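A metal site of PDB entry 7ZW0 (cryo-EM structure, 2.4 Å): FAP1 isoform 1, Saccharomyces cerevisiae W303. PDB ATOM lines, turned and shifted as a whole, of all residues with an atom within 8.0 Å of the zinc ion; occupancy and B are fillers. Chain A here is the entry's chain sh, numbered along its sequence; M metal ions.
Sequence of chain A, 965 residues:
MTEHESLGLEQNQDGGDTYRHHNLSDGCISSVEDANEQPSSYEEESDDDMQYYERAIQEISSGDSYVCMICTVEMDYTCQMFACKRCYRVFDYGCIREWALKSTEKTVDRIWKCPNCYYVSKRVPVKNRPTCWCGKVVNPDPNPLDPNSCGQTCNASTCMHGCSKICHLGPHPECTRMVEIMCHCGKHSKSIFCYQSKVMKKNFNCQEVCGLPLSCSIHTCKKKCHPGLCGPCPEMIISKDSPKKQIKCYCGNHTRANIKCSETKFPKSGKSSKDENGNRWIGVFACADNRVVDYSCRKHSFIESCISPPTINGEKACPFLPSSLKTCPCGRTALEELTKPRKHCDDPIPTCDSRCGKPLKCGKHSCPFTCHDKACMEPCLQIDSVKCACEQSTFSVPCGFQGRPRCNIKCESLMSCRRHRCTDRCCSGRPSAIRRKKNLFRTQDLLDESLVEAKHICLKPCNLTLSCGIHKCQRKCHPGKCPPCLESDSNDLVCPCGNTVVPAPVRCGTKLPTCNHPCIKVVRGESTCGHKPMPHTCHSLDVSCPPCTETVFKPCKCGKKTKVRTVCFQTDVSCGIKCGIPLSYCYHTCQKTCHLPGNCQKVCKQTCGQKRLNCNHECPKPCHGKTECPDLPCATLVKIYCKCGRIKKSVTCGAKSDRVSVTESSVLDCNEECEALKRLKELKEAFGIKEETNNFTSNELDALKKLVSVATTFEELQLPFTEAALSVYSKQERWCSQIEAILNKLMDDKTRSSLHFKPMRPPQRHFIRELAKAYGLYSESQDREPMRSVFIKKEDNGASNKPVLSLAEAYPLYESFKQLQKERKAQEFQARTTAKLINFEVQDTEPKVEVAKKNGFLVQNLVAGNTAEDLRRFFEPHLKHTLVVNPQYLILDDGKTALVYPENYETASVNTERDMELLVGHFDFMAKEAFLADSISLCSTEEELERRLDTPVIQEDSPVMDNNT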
ATOM      1  N   MET A  69     -20.377  -4.182  -2.455  1.00  0.00           N
ATOM      2  CA  MET A  69     -21.749  -3.781  -2.771  1.00  0.00           C
ATOM      3  C   MET A  69     -22.698  -3.571  -1.600  1.00  0.00           C
ATOM      4  O   MET A  69     -23.454  -2.603  -1.592  1.00  0.00           O
ATOM      5  CB  MET A  69     -22.360  -4.766  -3.768  1.00  0.00           C
ATOM      6  CG  MET A  69     -21.650  -4.784  -5.108  1.00  0.00           C
ATOM      7  SD  MET A  69     -22.466  -5.807  -6.352  1.00  0.00           S
ATOM      8  CE  MET A  69     -24.029  -4.953  -6.520  1.00  0.00           C
ATOM      9  N   PHE A  82     -15.369 -11.714  -1.271  1.00  0.00           N
ATOM     10  CA  PHE A  82     -16.153 -12.905  -1.634  1.00  0.00           C
ATOM     11  C   PHE A  82     -16.452 -12.918  -3.136  1.00  0.00           C
ATOM     12  O   PHE A  82     -16.833 -11.885  -3.692  1.00  0.00           O
ATOM     13  CB  PHE A  82     -17.457 -12.946  -0.868  1.00  0.00           C
ATOM     14  CG  PHE A  82     -18.341 -14.103  -1.247  1.00  0.00           C
ATOM     15  CD1 PHE A  82     -18.061 -15.373  -0.783  1.00  0.00           C
ATOM     16  CD2 PHE A  82     -19.447 -13.914  -2.048  1.00  0.00           C
ATOM     17  CE1 PHE A  82     -18.866 -16.449  -1.127  1.00  0.00           C
ATOM     18  CE2 PHE A  82     -20.251 -14.975  -2.408  1.00  0.00           C
ATOM     19  CZ  PHE A  82     -19.966 -16.238  -1.938  1.00  0.00           C
ATOM     20  N   ALA A  83     -16.270 -14.054  -3.788  1.00  0.00           N
ATOM     21  CA  ALA A  83     -16.473 -14.126  -5.230  1.00  0.00           C
ATOM     22  C   ALA A  83     -17.595 -15.066  -5.612  1.00  0.00           C
ATOM     23  O   ALA A  83     -17.713 -16.162  -5.064  1.00  0.00           O
ATOM     24  CB  ALA A  83     -15.187 -14.513  -5.926  1.00  0.00           C
ATOM     25  N   CYS A  84     -18.419 -14.655  -6.562  1.00  0.00           N
ATOM     26  CA  CYS A  84     -19.489 -15.519  -7.042  1.00  0.00           C
ATOM     27  C   CYS A  84     -19.229 -15.807  -8.500  1.00  0.00           C
ATOM     28  O   CYS A  84     -18.949 -14.892  -9.259  1.00  0.00           O
ATOM     29  CB  CYS A  84     -20.859 -14.862  -6.872  1.00  0.00           C
ATOM     30  SG  CYS A  84     -22.212 -15.758  -7.654  1.00  0.00           S
ATOM     31  N   LYS A  85     -19.315 -17.064  -8.906  1.00  0.00           N
ATOM     32  CA  LYS A  85     -18.991 -17.411 -10.279  1.00  0.00           C
ATOM     33  C   LYS A  85     -19.928 -16.748 -11.268  1.00  0.00           C
ATOM     34  O   LYS A  85     -19.504 -16.295 -12.320  1.00  0.00           O
ATOM     35  CB  LYS A  85     -19.020 -18.938 -10.472  1.00  0.00           C
ATOM     36  CG  LYS A  85     -17.787 -19.675  -9.949  1.00  0.00           C
ATOM     37  CD  LYS A  85     -17.846 -19.919  -8.445  1.00  0.00           C
ATOM     38  CE  LYS A  85     -16.862 -19.046  -7.699  1.00  0.00           C
ATOM     39  NZ  LYS A  85     -17.136 -19.035  -6.236  1.00  0.00           N
ATOM     40  N   ARG A  86     -21.207 -16.675 -10.931  1.00  0.00           N
ATOM     41  CA  ARG A  86     -22.176 -16.116 -11.860  1.00  0.00           C
ATOM     42  C   ARG A  86     -21.908 -14.638 -12.175  1.00  0.00           C
ATOM     43  O   ARG A  86     -21.974 -14.232 -13.337  1.00  0.00           O
ATOM     44  CB  ARG A  86     -23.600 -16.313 -11.327  1.00  0.00           C
ATOM     45  CG  ARG A  86     -24.680 -16.158 -12.389  1.00  0.00           C
ATOM     46  CD  ARG A  86     -24.538 -17.209 -13.471  1.00  0.00           C
ATOM     47  NE  ARG A  86     -25.264 -16.852 -14.686  1.00  0.00           N
ATOM     48  CZ  ARG A  86     -24.730 -16.198 -15.715  1.00  0.00           C
ATOM     49  NH1 ARG A  86     -23.458 -15.838 -15.679  1.00  0.00           N
ATOM     50  NH2 ARG A  86     -25.468 -15.906 -16.779  1.00  0.00           N
ATOM     51  N   CYS A  87     -21.589 -13.848 -11.159  1.00  0.00           N
ATOM     52  CA  CYS A  87     -21.319 -12.429 -11.388  1.00  0.00           C
ATOM     53  C   CYS A  87     -19.850 -12.070 -11.458  1.00  0.00           C
ATOM     54  O   CYS A  87     -19.518 -10.954 -11.860  1.00  0.00           O
ATOM     55  CB  CYS A  87     -21.952 -11.594 -10.282  1.00  0.00           C
ATOM     56  SG  CYS A  87     -21.130 -11.766  -8.685  1.00  0.00           S
ATOM     57  N   TYR A  88     -18.972 -12.996 -11.111  1.00  0.00           N
ATOM     58  CA  TYR A  88     -17.540 -12.697 -11.047  1.00  0.00           C
ATOM     59  C   TYR A  88     -17.254 -11.304 -10.500  1.00  0.00           C
ATOM     60  O   TYR A  88     -16.451 -10.554 -11.068  1.00  0.00           O
ATOM     61  CB  TYR A  88     -16.848 -12.949 -12.388  1.00  0.00           C
ATOM     62  CG  TYR A  88     -16.513 -14.405 -12.585  1.00  0.00           C
ATOM     63  CD1 TYR A  88     -15.831 -15.106 -11.598  1.00  0.00           C
ATOM     64  CD2 TYR A  88     -16.864 -15.071 -13.743  1.00  0.00           C
ATOM     65  CE1 TYR A  88     -15.520 -16.442 -11.764  1.00  0.00           C
ATOM     66  CE2 TYR A  88     -16.561 -16.405 -13.920  1.00  0.00           C
ATOM     67  CZ  TYR A  88     -15.893 -17.092 -12.919  1.00  0.00           C
ATOM     68  OH  TYR A  88     -15.585 -18.420 -13.090  1.00  0.00           O
ATOM     69  N   ARG A  89     -17.893 -10.955  -9.388  1.00  0.00           N
ATOM     70  CA  ARG A  89     -17.695  -9.660  -8.773  1.00  0.00           C
ATOM     71  C   ARG A  89     -17.332  -9.892  -7.312  1.00  0.00           C
ATOM     72  O   ARG A  89     -17.666 -10.939  -6.751  1.00  0.00           O
ATOM     73  CB  ARG A  89     -18.976  -8.830  -8.919  1.00  0.00           C
ATOM     74  CG  ARG A  89     -19.179  -7.690  -7.935  1.00  0.00           C
ATOM     75  CD  ARG A  89     -18.888  -6.339  -8.560  1.00  0.00           C
ATOM     76  NE  ARG A  89     -18.954  -5.263  -7.576  1.00  0.00           N
ATOM     77  CZ  ARG A  89     -18.821  -3.968  -7.865  1.00  0.00           C
ATOM     78  NH1 ARG A  89     -18.632  -3.591  -9.121  1.00  0.00           N
ATOM     79  NH2 ARG A  89     -18.879  -3.062  -6.900  1.00  0.00           N
ATOM     80  N   VAL A  90     -16.650  -8.948  -6.682  1.00  0.00           N
ATOM     81  CA  VAL A  90     -16.219  -9.122  -5.297  1.00  0.00           C
ATOM     82  C   VAL A  90     -16.805  -8.131  -4.299  1.00  0.00           C
ATOM     83  O   VAL A  90     -16.916  -6.932  -4.590  1.00  0.00           O
ATOM     84  CB  VAL A  90     -14.688  -9.165  -5.209  1.00  0.00           C
ATOM     85  CG1 VAL A  90     -14.173  -8.662  -3.883  1.00  0.00           C
ATOM     86  CG2 VAL A  90     -14.203 -10.572  -5.476  1.00  0.00           C
ATOM     87  N   PHE A  91     -17.236  -8.622  -3.140  1.00  0.00           N
ATOM     88  CA  PHE A  91     -17.783  -7.753  -2.104  1.00  0.00           C
ATOM     89  C   PHE A  91     -17.020  -8.091  -0.842  1.00  0.00           C
ATOM     90  O   PHE A  91     -16.297  -9.075  -0.810  1.00  0.00           O
ATOM     91  CB  PHE A  91     -19.268  -8.047  -1.893  1.00  0.00           C
ATOM     92  CG  PHE A  91     -19.895  -8.840  -2.997  1.00  0.00           C
ATOM     93  CD1 PHE A  91     -19.855 -10.232  -2.974  1.00  0.00           C
ATOM     94  CD2 PHE A  91     -20.522  -8.208  -4.057  1.00  0.00           C
ATOM     95  CE1 PHE A  91     -20.432 -10.968  -3.998  1.00  0.00           C
ATOM     96  CE2 PHE A  91     -21.101  -8.937  -5.069  1.00  0.00           C
ATOM     97  CZ  PHE A  91     -21.049 -10.324  -5.046  1.00  0.00           C
ATOM     98  N   ILE A  96     -21.197  -9.349   2.670  1.00  0.00           N
ATOM     99  CA  ILE A  96     -22.046 -10.209   1.869  1.00  0.00           C
ATOM    100  C   ILE A  96     -22.685 -11.312   2.725  1.00  0.00           C
ATOM    101  O   ILE A  96     -23.789 -11.761   2.418  1.00  0.00           O
ATOM    102  CB  ILE A  96     -21.291 -10.794   0.652  1.00  0.00           C
ATOM    103  CG1 ILE A  96     -22.272 -11.216  -0.446  1.00  0.00           C
ATOM    104  CG2 ILE A  96     -20.424 -11.987   1.040  1.00  0.00           C
ATOM    105  CD1 ILE A  96     -23.098 -10.075  -0.992  1.00  0.00           C
ATOM    106  N   TRP A 112     -29.710 -17.801   0.024  1.00  0.00           N
ATOM    107  CA  TRP A 112     -29.004 -16.525  -0.078  1.00  0.00           C
ATOM    108  C   TRP A 112     -28.934 -16.017  -1.525  1.00  0.00           C
ATOM    109  O   TRP A 112     -28.879 -16.812  -2.449  1.00  0.00           O
ATOM    110  CB  TRP A 112     -27.606 -16.652   0.529  1.00  0.00           C
ATOM    111  CG  TRP A 112     -26.502 -16.796  -0.460  1.00  0.00           C
ATOM    112  CD1 TRP A 112     -26.085 -17.939  -1.069  1.00  0.00           C
ATOM    113  CD2 TRP A 112     -25.651 -15.744  -0.957  1.00  0.00           C
ATOM    114  NE1 TRP A 112     -25.033 -17.665  -1.906  1.00  0.00           N
ATOM    115  CE2 TRP A 112     -24.754 -16.327  -1.859  1.00  0.00           C
ATOM    116  CE3 TRP A 112     -25.577 -14.369  -0.719  1.00  0.00           C
ATOM    117  CZ2 TRP A 112     -23.789 -15.590  -2.527  1.00  0.00           C
ATOM    118  CZ3 TRP A 112     -24.622 -13.646  -1.382  1.00  0.00           C
ATOM    119  CH2 TRP A 112     -23.734 -14.242  -2.279  1.00  0.00           C
ATOM    120  N   LYS A 113     -28.922 -14.697  -1.726  1.00  0.00           N
ATOM    121  CA  LYS A 113     -28.936 -14.159  -3.102  1.00  0.00           C
ATOM    122  C   LYS A 113     -27.728 -13.284  -3.410  1.00  0.00           C
ATOM    123  O   LYS A 113     -27.326 -12.483  -2.582  1.00  0.00           O
ATOM    124  CB  LYS A 113     -30.224 -13.361  -3.338  1.00  0.00           C
ATOM    125  CG  LYS A 113     -30.454 -12.979  -4.794  1.00  0.00           C
ATOM    126  CD  LYS A 113     -31.909 -12.634  -5.038  1.00  0.00           C
ATOM    127  CE  LYS A 113     -32.209 -12.627  -6.526  1.00  0.00           C
ATOM    128  NZ  LYS A 113     -33.670 -12.459  -6.789  1.00  0.00           N
ATOM    129  N   CYS A 114     -27.163 -13.433  -4.590  1.00  0.00           N
ATOM    130  CA  CYS A 114     -26.045 -12.598  -4.980  1.00  0.00           C
ATOM    131  C   CYS A 114     -26.550 -11.420  -5.783  1.00  0.00           C
ATOM    132  O   CYS A 114     -27.141 -11.607  -6.840  1.00  0.00           O
ATOM    133  CB  CYS A 114     -25.037 -13.393  -5.797  1.00  0.00           C
ATOM    134  SG  CYS A 114     -23.586 -12.434  -6.267  1.00  0.00           S
ATOM    135  N   PRO A 115     -26.312 -10.193  -5.310  1.00  0.00           N
ATOM    136  CA  PRO A 115     -26.858  -8.997  -5.970  1.00  0.00           C
ATOM    137  C   PRO A 115     -26.372  -8.670  -7.381  1.00  0.00           C
ATOM    138  O   PRO A 115     -27.201  -8.286  -8.206  1.00  0.00           O
ATOM    139  CB  PRO A 115     -26.435  -7.850  -5.042  1.00  0.00           C
ATOM    140  CG  PRO A 115     -26.066  -8.502  -3.742  1.00  0.00           C
ATOM    141  CD  PRO A 115     -25.531  -9.847  -4.108  1.00  0.00           C
ATOM    142  N   ASN A 116     -25.088  -8.807  -7.660  1.00  0.00           N
ATOM    143  CA  ASN A 116     -24.590  -8.391  -8.975  1.00  0.00           C
ATOM    144  C   ASN A 116     -25.190  -9.191 -10.110  1.00  0.00           C
ATOM    145  O   ASN A 116     -25.560  -8.631 -11.146  1.00  0.00           O
ATOM    146  CB  ASN A 116     -23.063  -8.455  -9.023  1.00  0.00           C
ATOM    147  CG  ASN A 116     -22.485  -7.603 -10.148  1.00  0.00           C
ATOM    148  OD1 ASN A 116     -22.789  -6.412 -10.247  1.00  0.00           O
ATOM    149  ND2 ASN A 116     -21.644  -8.202 -10.973  1.00  0.00           N
ATOM    150  N   CYS A 117     -25.308 -10.498  -9.933  1.00  0.00           N
ATOM    151  CA  CYS A 117     -25.943 -11.328 -10.947  1.00  0.00           C
ATOM    152  C   CYS A 117     -27.407 -11.499 -10.631  1.00  0.00           C
ATOM    153  O   CYS A 117     -28.118 -12.186 -11.372  1.00  0.00           O
ATOM    154  CB  CYS A 117     -25.265 -12.689 -11.030  1.00  0.00           C
ATOM    155  SG  CYS A 117     -24.901 -13.408  -9.424  1.00  0.00           S
ATOM    156  N   TYR A 118     -27.863 -10.903  -9.534  1.00  0.00           N
ATOM    157  CA  TYR A 118     -29.250 -11.058  -9.102  1.00  0.00           C
ATOM    158  C   TYR A 118     -29.567 -12.536  -9.146  1.00  0.00           C
ATOM    159  O   TYR A 118     -30.610 -12.942  -9.653  1.00  0.00           O
ATOM    160  CB  TYR A 118     -30.201 -10.246  -9.999  1.00  0.00           C
ATOM    161  CG  TYR A 118     -31.504  -9.890  -9.340  1.00  0.00           C
ATOM    162  CD1 TYR A 118     -31.539  -9.129  -8.176  1.00  0.00           C
ATOM    163  CD2 TYR A 118     -32.714 -10.304  -9.884  1.00  0.00           C
ATOM    164  CE1 TYR A 118     -32.733  -8.807  -7.572  1.00  0.00           C
ATOM    165  CE2 TYR A 118     -33.917  -9.980  -9.290  1.00  0.00           C
ATOM    166  CZ  TYR A 118     -33.919  -9.221  -8.134  1.00  0.00           C
ATOM    167  OH  TYR A 118     -35.117  -8.891  -7.534  1.00  0.00           O
ATOM    168  N   TYR A 119     -28.662 -13.354  -8.620  1.00  0.00           N
ATOM    169  CA  TYR A 119     -28.845 -14.800  -8.688  1.00  0.00           C
ATOM    170  C   TYR A 119     -28.852 -15.414  -7.319  1.00  0.00           C
ATOM    171  O   TYR A 119     -27.944 -15.181  -6.524  1.00  0.00           O
ATOM    172  CB  TYR A 119     -27.767 -15.407  -9.599  1.00  0.00           C
ATOM    173  CG  TYR A 119     -27.101 -16.689  -9.126  1.00  0.00           C
ATOM    174  CD1 TYR A 119     -25.963 -16.658  -8.337  1.00  0.00           C
ATOM    175  CD2 TYR A 119     -27.584 -17.928  -9.522  1.00  0.00           C
ATOM    176  CE1 TYR A 119     -25.345 -17.815  -7.914  1.00  0.00           C
ATOM    177  CE2 TYR A 119     -26.971 -19.091  -9.105  1.00  0.00           C
ATOM    178  CZ  TYR A 119     -25.862 -19.029  -8.306  1.00  0.00           C
ATOM    179  OH  TYR A 119     -25.244 -20.186  -7.882  1.00  0.00           O
ATOM    180  N   VAL A 120     -29.893 -16.177  -7.011  1.00  0.00           N
ATOM    181  CA  VAL A 120     -29.949 -16.848  -5.722  1.00  0.00           C
ATOM    182  C   VAL A 120     -29.074 -18.081  -5.717  1.00  0.00           C
ATOM    183  O   VAL A 120     -28.964 -18.773  -6.719  1.00  0.00           O
ATOM    184  CB  VAL A 120     -31.390 -17.259  -5.386  1.00  0.00           C
ATOM    185  CG1 VAL A 120     -31.832 -16.615  -4.075  1.00  0.00           C
ATOM    186  CG2 VAL A 120     -32.322 -16.862  -6.508  1.00  0.00           C
ATOM    187  N   SER A 121     -28.461 -18.375  -4.584  1.00  0.00           N
ATOM    188  CA  SER A 121     -27.652 -19.586  -4.452  1.00  0.00           C
ATOM    189  C   SER A 121     -28.089 -20.274  -3.181  1.00  0.00           C
ATOM    190  O   SER A 121     -28.781 -19.661  -2.359  1.00  0.00           O
ATOM    191  CB  SER A 121     -26.157 -19.271  -4.469  1.00  0.00           C
ATOM    192  OG  SER A 121     -25.380 -20.460  -4.444  1.00  0.00           O
HETATM  193 ZN    ZN M   1     -22.777 -13.314  -7.929  1.00  0.00          ZN
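N of Cys 114 lies within hydrogen-bond range of O of Tyr 119, at 2.7 Å.
The side-chain sulfur (SG) of Cys 84 lies close to the backbone NH (N) of Arg 86.
The side-chain sulfur of Cys 87 sits close to the backbone NH of Arg 89 (3.4 Å).
Four residues have an atom within 4 Å of the zinc ion: Cys 84, Cys 87, Cys 114 and Cys 117.
The zinc ion is bound by SG of Cys 114, SG of Cys 87, SG of Cys 84 and SG of Cys 117.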
